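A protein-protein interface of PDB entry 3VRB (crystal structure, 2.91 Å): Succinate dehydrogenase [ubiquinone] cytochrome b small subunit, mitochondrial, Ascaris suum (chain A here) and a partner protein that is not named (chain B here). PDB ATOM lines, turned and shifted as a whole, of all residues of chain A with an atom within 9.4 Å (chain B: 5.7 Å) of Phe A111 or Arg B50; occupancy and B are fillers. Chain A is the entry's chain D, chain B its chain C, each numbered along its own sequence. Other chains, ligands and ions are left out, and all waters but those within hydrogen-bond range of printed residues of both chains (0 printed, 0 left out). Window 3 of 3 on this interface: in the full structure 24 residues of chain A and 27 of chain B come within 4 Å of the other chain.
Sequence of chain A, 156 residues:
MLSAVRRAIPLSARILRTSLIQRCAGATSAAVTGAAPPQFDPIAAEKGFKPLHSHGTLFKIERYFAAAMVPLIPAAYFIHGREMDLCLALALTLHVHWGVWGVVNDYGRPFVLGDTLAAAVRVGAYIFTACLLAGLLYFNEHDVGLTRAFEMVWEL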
ATOM      1  N   ASP A 106       7.194 -14.337 -33.738  1.00  0.00           N
ATOM      2  CA  ASP A 106       6.166 -15.332 -33.526  1.00  0.00           C
ATOM      3  C   ASP A 106       6.706 -16.674 -33.979  1.00  0.00           C
ATOM      4  O   ASP A 106       7.204 -17.444 -33.167  1.00  0.00           O
ATOM      5  CB  ASP A 106       4.875 -14.944 -34.261  1.00  0.00           C
ATOM      6  CG  ASP A 106       4.252 -13.652 -33.707  1.00  0.00           C
ATOM      7  OD1 ASP A 106       4.393 -13.396 -32.490  1.00  0.00           O
ATOM      8  OD2 ASP A 106       3.624 -12.886 -34.474  1.00  0.00           O
ATOM      9  N   TYR A 107       6.662 -16.935 -35.278  1.00  0.00           N
ATOM     10  CA  TYR A 107       6.908 -18.283 -35.770  1.00  0.00           C
ATOM     11  C   TYR A 107       8.340 -18.761 -35.615  1.00  0.00           C
ATOM     12  O   TYR A 107       8.584 -19.964 -35.512  1.00  0.00           O
ATOM     13  CB  TYR A 107       6.402 -18.425 -37.195  1.00  0.00           C
ATOM     14  CG  TYR A 107       4.996 -17.953 -37.270  1.00  0.00           C
ATOM     15  CD1 TYR A 107       4.718 -16.631 -37.573  1.00  0.00           C
ATOM     16  CD2 TYR A 107       3.942 -18.800 -36.967  1.00  0.00           C
ATOM     17  CE1 TYR A 107       3.433 -16.172 -37.613  1.00  0.00           C
ATOM     18  CE2 TYR A 107       2.641 -18.351 -37.008  1.00  0.00           C
ATOM     19  CZ  TYR A 107       2.397 -17.031 -37.329  1.00  0.00           C
ATOM     20  OH  TYR A 107       1.117 -16.545 -37.371  1.00  0.00           O
ATOM     21  N   GLY A 108       9.280 -17.836 -35.565  1.00  0.00           N
ATOM     22  CA  GLY A 108      10.662 -18.231 -35.508  1.00  0.00           C
ATOM     23  C   GLY A 108      11.178 -18.050 -34.104  1.00  0.00           C
ATOM     24  O   GLY A 108      11.526 -16.942 -33.696  1.00  0.00           O
ATOM     25  N   ARG A 109      11.236 -19.136 -33.351  1.00  0.00           N
ATOM     26  CA  ARG A 109      11.621 -19.022 -31.958  1.00  0.00           C
ATOM     27  C   ARG A 109      12.476 -20.182 -31.444  1.00  0.00           C
ATOM     28  O   ARG A 109      12.348 -21.331 -31.893  1.00  0.00           O
ATOM     29  CB  ARG A 109      10.395 -18.735 -31.051  1.00  0.00           C
ATOM     30  CG  ARG A 109       9.075 -19.430 -31.443  1.00  0.00           C
ATOM     31  CD  ARG A 109       9.245 -20.917 -31.472  1.00  0.00           C
ATOM     32  NE  ARG A 109       8.127 -21.606 -32.083  1.00  0.00           N
ATOM     33  CZ  ARG A 109       7.225 -22.308 -31.405  1.00  0.00           C
ATOM     34  NH1 ARG A 109       6.259 -22.923 -32.061  1.00  0.00           N
ATOM     35  NH2 ARG A 109       7.283 -22.399 -30.079  1.00  0.00           N
ATOM     36  N   PRO A 110      13.345 -19.861 -30.476  1.00  0.00           N
ATOM     37  CA  PRO A 110      14.434 -20.650 -29.949  1.00  0.00           C
ATOM     38  C   PRO A 110      14.074 -22.081 -29.604  1.00  0.00           C
ATOM     39  O   PRO A 110      14.802 -22.984 -30.009  1.00  0.00           O
ATOM     40  CB  PRO A 110      14.830 -19.885 -28.694  1.00  0.00           C
ATOM     41  CG  PRO A 110      13.664 -18.991 -28.403  1.00  0.00           C
ATOM     42  CD  PRO A 110      13.231 -18.595 -29.739  1.00  0.00           C
ATOM     43  N   PHE A 111      12.977 -22.313 -28.879  1.00  0.00           N
ATOM     44  CA  PHE A 111      12.675 -23.681 -28.438  1.00  0.00           C
ATOM     45  C   PHE A 111      12.730 -24.681 -29.592  1.00  0.00           C
ATOM     46  O   PHE A 111      13.298 -25.763 -29.462  1.00  0.00           O
ATOM     47  CB  PHE A 111      11.335 -23.783 -27.703  1.00  0.00           C
ATOM     48  CG  PHE A 111      11.091 -25.146 -27.075  1.00  0.00           C
ATOM     49  CD1 PHE A 111      11.811 -25.555 -25.954  1.00  0.00           C
ATOM     50  CD2 PHE A 111      10.147 -26.026 -27.614  1.00  0.00           C
ATOM     51  CE1 PHE A 111      11.594 -26.808 -25.386  1.00  0.00           C
ATOM     52  CE2 PHE A 111       9.920 -27.287 -27.041  1.00  0.00           C
ATOM     53  CZ  PHE A 111      10.646 -27.675 -25.930  1.00  0.00           C
ATOM     54  N   VAL A 112      12.160 -24.289 -30.724  1.00  0.00           N
ATOM     55  CA  VAL A 112      12.085 -25.160 -31.880  1.00  0.00           C
ATOM     56  C   VAL A 112      13.332 -25.053 -32.752  1.00  0.00           C
ATOM     57  O   VAL A 112      13.777 -26.049 -33.306  1.00  0.00           O
ATOM     58  CB  VAL A 112      10.809 -24.873 -32.701  1.00  0.00           C
ATOM     59  CG1 VAL A 112      11.003 -25.228 -34.159  1.00  0.00           C
ATOM     60  CG2 VAL A 112       9.619 -25.623 -32.114  1.00  0.00           C
ATOM     61  N   LEU A 113      13.906 -23.859 -32.861  1.00  0.00           N
ATOM     62  CA  LEU A 113      14.997 -23.638 -33.816  1.00  0.00           C
ATOM     63  C   LEU A 113      16.406 -23.809 -33.260  1.00  0.00           C
ATOM     64  O   LEU A 113      17.336 -24.019 -34.028  1.00  0.00           O
ATOM     65  CB  LEU A 113      14.909 -22.242 -34.432  1.00  0.00           C
ATOM     66  CG  LEU A 113      13.651 -21.827 -35.181  1.00  0.00           C
ATOM     67  CD1 LEU A 113      13.730 -20.356 -35.507  1.00  0.00           C
ATOM     68  CD2 LEU A 113      13.462 -22.645 -36.429  1.00  0.00           C
ATOM     69  N   GLY A 114      16.570 -23.688 -31.944  1.00  0.00           N
ATOM     70  CA  GLY A 114      17.896 -23.605 -31.327  1.00  0.00           C
ATOM     71  C   GLY A 114      18.393 -22.188 -31.517  1.00  0.00           C
ATOM     72  O   GLY A 114      18.164 -21.609 -32.584  1.00  0.00           O
ATOM     73  N   ASP A 115      19.079 -21.637 -30.504  1.00  0.00           N
ATOM     74  CA  ASP A 115      19.356 -20.174 -30.413  1.00  0.00           C
ATOM     75  C   ASP A 115      20.133 -19.561 -31.585  1.00  0.00           C
ATOM     76  O   ASP A 115      19.763 -18.494 -32.079  1.00  0.00           O
ATOM     77  CB  ASP A 115      20.003 -19.778 -29.055  1.00  0.00           C
ATOM     78  CG  ASP A 115      18.957 -19.381 -27.952  1.00  0.00           C
ATOM     79  OD1 ASP A 115      19.331 -19.266 -26.752  1.00  0.00           O
ATOM     80  OD2 ASP A 115      17.762 -19.173 -28.274  1.00  0.00           O
ATOM     81  N   THR A 116      21.188 -20.245 -32.035  1.00  0.00           N
ATOM     82  CA  THR A 116      22.097 -19.689 -33.060  1.00  0.00           C
ATOM     83  C   THR A 116      21.413 -19.486 -34.431  1.00  0.00           C
ATOM     84  O   THR A 116      21.777 -18.582 -35.178  1.00  0.00           O
ATOM     85  CB  THR A 116      23.462 -20.468 -33.180  1.00  0.00           C
ATOM     86  OG1 THR A 116      23.575 -21.088 -34.472  1.00  0.00           O
ATOM     87  CG2 THR A 116      23.642 -21.514 -32.044  1.00  0.00           C
ATOM     88  N   ALA A 118      18.073 -18.942 -34.625  1.00  0.00           N
ATOM     89  CA  ALA A 118      17.010 -17.983 -34.321  1.00  0.00           C
ATOM     90  C   ALA A 118      17.481 -16.546 -34.389  1.00  0.00           C
ATOM     91  O   ALA A 118      16.682 -15.635 -34.587  1.00  0.00           O
ATOM     92  CB  ALA A 118      16.470 -18.244 -32.964  1.00  0.00           C
ATOM     93  N   ARG A 122      16.112 -13.476 -37.185  1.00  0.00           N
ATOM     94  CA  ARG A 122      16.032 -12.106 -36.693  1.00  0.00           C
ATOM     95  C   ARG A 122      16.879 -11.164 -37.543  1.00  0.00           C
ATOM     96  O   ARG A 122      16.582  -9.981 -37.642  1.00  0.00           O
ATOM     97  CB  ARG A 122      16.522 -12.054 -35.247  1.00  0.00           C
ATOM     98  CG  ARG A 122      15.446 -11.918 -34.166  1.00  0.00           C
ATOM     99  CD  ARG A 122      15.866 -12.575 -32.826  1.00  0.00           C
ATOM    100  NE  ARG A 122      15.435 -13.975 -32.765  1.00  0.00           N
ATOM    101  CZ  ARG A 122      14.176 -14.389 -32.973  1.00  0.00           C
ATOM    102  NH1 ARG A 122      13.211 -13.517 -33.266  1.00  0.00           N
ATOM    103  NH2 ARG A 122      13.871 -15.683 -32.899  1.00  0.00           N
ATOM    104  N   TRP B  43      11.840 -20.572 -19.548  1.00  0.00           N
ATOM    105  CA  TRP B  43      12.826 -21.272 -20.337  1.00  0.00           C
ATOM    106  C   TRP B  43      13.171 -22.627 -19.687  1.00  0.00           C
ATOM    107  O   TRP B  43      12.967 -23.689 -20.292  1.00  0.00           O
ATOM    108  CB  TRP B  43      14.077 -20.410 -20.573  1.00  0.00           C
ATOM    109  CG  TRP B  43      15.053 -21.124 -21.486  1.00  0.00           C
ATOM    110  CD1 TRP B  43      16.233 -21.742 -21.129  1.00  0.00           C
ATOM    111  CD2 TRP B  43      14.895 -21.354 -22.886  1.00  0.00           C
ATOM    112  NE1 TRP B  43      16.811 -22.316 -22.224  1.00  0.00           N
ATOM    113  CE2 TRP B  43      16.006 -22.095 -23.315  1.00  0.00           C
ATOM    114  CE3 TRP B  43      13.920 -20.998 -23.824  1.00  0.00           C
ATOM    115  CZ2 TRP B  43      16.170 -22.477 -24.646  1.00  0.00           C
ATOM    116  CZ3 TRP B  43      14.087 -21.381 -25.141  1.00  0.00           C
ATOM    117  CH2 TRP B  43      15.197 -22.111 -25.536  1.00  0.00           C
ATOM    118  N   TYR B  45      11.781 -24.285 -17.598  1.00  0.00           N
ATOM    119  CA  TYR B  45      10.622 -25.150 -17.569  1.00  0.00           C
ATOM    120  C   TYR B  45      10.556 -25.973 -18.852  1.00  0.00           C
ATOM    121  O   TYR B  45      10.340 -27.180 -18.832  1.00  0.00           O
ATOM    122  CB  TYR B  45       9.329 -24.357 -17.341  1.00  0.00           C
ATOM    123  CG  TYR B  45       8.102 -25.166 -17.671  1.00  0.00           C
ATOM    124  CD1 TYR B  45       7.701 -26.225 -16.865  1.00  0.00           C
ATOM    125  CD2 TYR B  45       7.368 -24.908 -18.821  1.00  0.00           C
ATOM    126  CE1 TYR B  45       6.586 -26.987 -17.189  1.00  0.00           C
ATOM    127  CE2 TYR B  45       6.259 -25.673 -19.153  1.00  0.00           C
ATOM    128  CZ  TYR B  45       5.877 -26.706 -18.331  1.00  0.00           C
ATOM    129  OH  TYR B  45       4.781 -27.452 -18.672  1.00  0.00           O
ATOM    130  N   LEU B  46      10.768 -25.321 -19.979  1.00  0.00           N
ATOM    131  CA  LEU B  46      10.627 -26.022 -21.234  1.00  0.00           C
ATOM    132  C   LEU B  46      11.780 -26.968 -21.373  1.00  0.00           C
ATOM    133  O   LEU B  46      11.596 -28.086 -21.818  1.00  0.00           O
ATOM    134  CB  LEU B  46      10.499 -25.057 -22.416  1.00  0.00           C
ATOM    135  CG  LEU B  46       9.265 -24.117 -22.452  1.00  0.00           C
ATOM    136  CD1 LEU B  46       9.427 -23.078 -23.542  1.00  0.00           C
ATOM    137  CD2 LEU B  46       7.920 -24.815 -22.635  1.00  0.00           C
ATOM    138  N   MET B  47      12.958 -26.550 -20.929  1.00  0.00           N
ATOM    139  CA  MET B  47      14.099 -27.472 -20.885  1.00  0.00           C
ATOM    140  C   MET B  47      13.776 -28.728 -20.064  1.00  0.00           C
ATOM    141  O   MET B  47      13.949 -29.859 -20.540  1.00  0.00           O
ATOM    142  CB  MET B  47      15.364 -26.787 -20.366  1.00  0.00           C
ATOM    143  CG  MET B  47      16.111 -25.955 -21.415  1.00  0.00           C
ATOM    144  SD  MET B  47      16.168 -26.607 -23.129  1.00  0.00           S
ATOM    145  CE  MET B  47      14.993 -25.538 -23.997  1.00  0.00           C
ATOM    146  N   ARG B  48      13.290 -28.511 -18.841  1.00  0.00           N
ATOM    147  CA  ARG B  48      12.822 -29.589 -17.996  1.00  0.00           C
ATOM    148  C   ARG B  48      11.813 -30.492 -18.732  1.00  0.00           C
ATOM    149  O   ARG B  48      11.911 -31.727 -18.688  1.00  0.00           O
ATOM    150  CB  ARG B  48      12.218 -29.019 -16.712  1.00  0.00           C
ATOM    151  CG  ARG B  48      13.213 -28.891 -15.579  1.00  0.00           C
ATOM    152  CD  ARG B  48      12.559 -28.464 -14.282  1.00  0.00           C
ATOM    153  NE  ARG B  48      12.512 -27.008 -14.139  1.00  0.00           N
ATOM    154  CZ  ARG B  48      11.393 -26.283 -14.065  1.00  0.00           C
ATOM    155  NH1 ARG B  48      10.200 -26.883 -14.127  1.00  0.00           N
ATOM    156  NH2 ARG B  48      11.467 -24.955 -13.919  1.00  0.00           N
ATOM    157  N   GLN B  49      10.866 -29.875 -19.429  1.00  0.00           N
ATOM    158  CA  GLN B  49       9.757 -30.625 -19.956  1.00  0.00           C
ATOM    159  C   GLN B  49      10.146 -31.403 -21.188  1.00  0.00           C
ATOM    160  O   GLN B  49       9.596 -32.469 -21.457  1.00  0.00           O
ATOM    161  CB  GLN B  49       8.572 -29.707 -20.228  1.00  0.00           C
ATOM    162  CG  GLN B  49       7.928 -29.112 -18.969  1.00  0.00           C
ATOM    163  CD  GLN B  49       7.381 -30.159 -17.997  1.00  0.00           C
ATOM    164  OE1 GLN B  49       6.769 -31.158 -18.400  1.00  0.00           O
ATOM    165  NE2 GLN B  49       7.598 -29.929 -16.706  1.00  0.00           N
ATOM    166  N   ARG B  50      11.106 -30.885 -21.939  1.00  0.00           N
ATOM    167  CA  ARG B  50      11.593 -31.621 -23.087  1.00  0.00           C
ATOM    168  C   ARG B  50      12.531 -32.720 -22.584  1.00  0.00           C
ATOM    169  O   ARG B  50      12.605 -33.811 -23.162  1.00  0.00           O
ATOM    170  CB  ARG B  50      12.264 -30.694 -24.110  1.00  0.00           C
ATOM    171  CG  ARG B  50      13.768 -30.460 -23.936  1.00  0.00           C
ATOM    172  CD  ARG B  50      14.576 -30.754 -25.235  1.00  0.00           C
ATOM    173  NE  ARG B  50      13.994 -30.202 -26.475  1.00  0.00           N
ATOM    174  CZ  ARG B  50      14.249 -28.991 -26.984  1.00  0.00           C
ATOM    175  NH1 ARG B  50      15.084 -28.151 -26.373  1.00  0.00           N
ATOM    176  NH2 ARG B  50      13.653 -28.616 -28.114  1.00  0.00           N
ATOM    177  N   ALA B  51      13.215 -32.425 -21.481  1.00  0.00           N
ATOM    178  CA  ALA B  51      14.079 -33.393 -20.816  1.00  0.00           C
ATOM    179  C   ALA B  51      13.342 -34.690 -20.409  1.00  0.00           C
ATOM    180  O   ALA B  51      13.974 -35.729 -20.189  1.00  0.00           O
ATOM    181  CB  ALA B  51      14.746 -32.755 -19.609  1.00  0.00           C
ATOM    182  N   LEU B  52      12.014 -34.634 -20.309  1.00  0.00           N
ATOM    183  CA  LEU B  52      11.264 -35.800 -19.884  1.00  0.00           C
ATOM    184  C   LEU B  52      10.484 -36.361 -21.050  1.00  0.00           C
ATOM    185  O   LEU B  52       9.590 -37.185 -20.867  1.00  0.00           O
ATOM    186  CB  LEU B  52      10.315 -35.471 -18.720  1.00  0.00           C
ATOM    187  CG  LEU B  52      10.657 -34.541 -17.538  1.00  0.00           C
ATOM    188  CD1 LEU B  52       9.544 -34.688 -16.516  1.00  0.00           C
ATOM    189  CD2 LEU B  52      12.046 -34.740 -16.876  1.00  0.00           C
ATOM    190  N   LYS B  53      10.826 -35.925 -22.256  1.00  0.00           N
ATOM    191  CA  LYS B  53      10.196 -36.456 -23.465  1.00  0.00           C
ATOM    192  C   LYS B  53       8.703 -36.593 -23.244  1.00  0.00           C
ATOM    193  O   LYS B  53       8.119 -37.664 -23.420  1.00  0.00           O
ATOM    194  CB  LYS B  53      10.797 -37.813 -23.881  1.00  0.00           C
ATOM    195  CG  LYS B  53      12.274 -38.056 -23.486  1.00  0.00           C
ATOM    196  CD  LYS B  53      12.374 -38.823 -22.147  1.00  0.00           C
ATOM    197  CE  LYS B  53      13.705 -38.587 -21.403  1.00  0.00           C
ATOM    198  NZ  LYS B  53      14.884 -39.329 -21.970  1.00  0.00           N
ATOM    199  N   ARG B  54       8.102 -35.496 -22.806  1.00  0.00           N
ATOM    200  CA  ARG B  54       6.666 -35.421 -22.649  1.00  0.00           C
ATOM    201  C   ARG B  54       6.072 -34.855 -23.932  1.00  0.00           C
ATOM    202  O   ARG B  54       6.707 -34.034 -24.591  1.00  0.00           O
ATOM    203  CB  ARG B  54       6.320 -34.561 -21.449  1.00  0.00           C
ATOM    204  CG  ARG B  54       6.459 -35.285 -20.124  1.00  0.00           C
ATOM    205  CD  ARG B  54       5.879 -34.393 -19.065  1.00  0.00           C
ATOM    206  NE  ARG B  54       5.682 -35.025 -17.767  1.00  0.00           N
ATOM    207  CZ  ARG B  54       5.798 -34.361 -16.617  1.00  0.00           C
ATOM    208  NH1 ARG B  54       6.132 -33.074 -16.652  1.00  0.00           N
ATOM    209  NH2 ARG B  54       5.614 -34.972 -15.442  1.00  0.00           N
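Trp B43 touches Pro A110.
Phe A111 touches Leu B46.
Met B47 touches Phe A111.
SD of Met B47 sits close to NH1 of Arg B50 (3.8 Å).
Printed residues of chain A that touch a printed residue of chain B: Pro A110 and Phe A111.
Among the printed residues, 4 pairs touch across the chains.
Among the printed residues, no Asp or Glu carboxylate lies within 4 Å of a Lys or Arg side-chain nitrogen of the other chain.
NH2 of Arg B50 sits at hydrogen-bond distance from O of Phe A111, 3.2 Å away.
Printed residues of chain B within 4 Å of Phe A111: Leu B46, Met B47 and Arg B50.
Arg B50 touches one residue of chain A.
No residue of chain A comes within 4 Å of Ala B51.
Printed residues of chain A within 4 Å of Met B47: Phe A111 (3.7 Å).
Printed residues of chain B within 4 Å of Pro A110: Trp B43.
Printed residues of chain A within 4 Å of Trp B43: Pro A110 (3.9 Å).
Of the printed residues of chain A, Leu B46 touches Phe A111 (3.6 Å).
Leu A113 touches none of the printed residues of chain B.
Gly A108 touches none of the printed residues of chain B.
The nearest printed residue of chain A that does not touch Met B47 is Pro A110 (6.5 Å).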
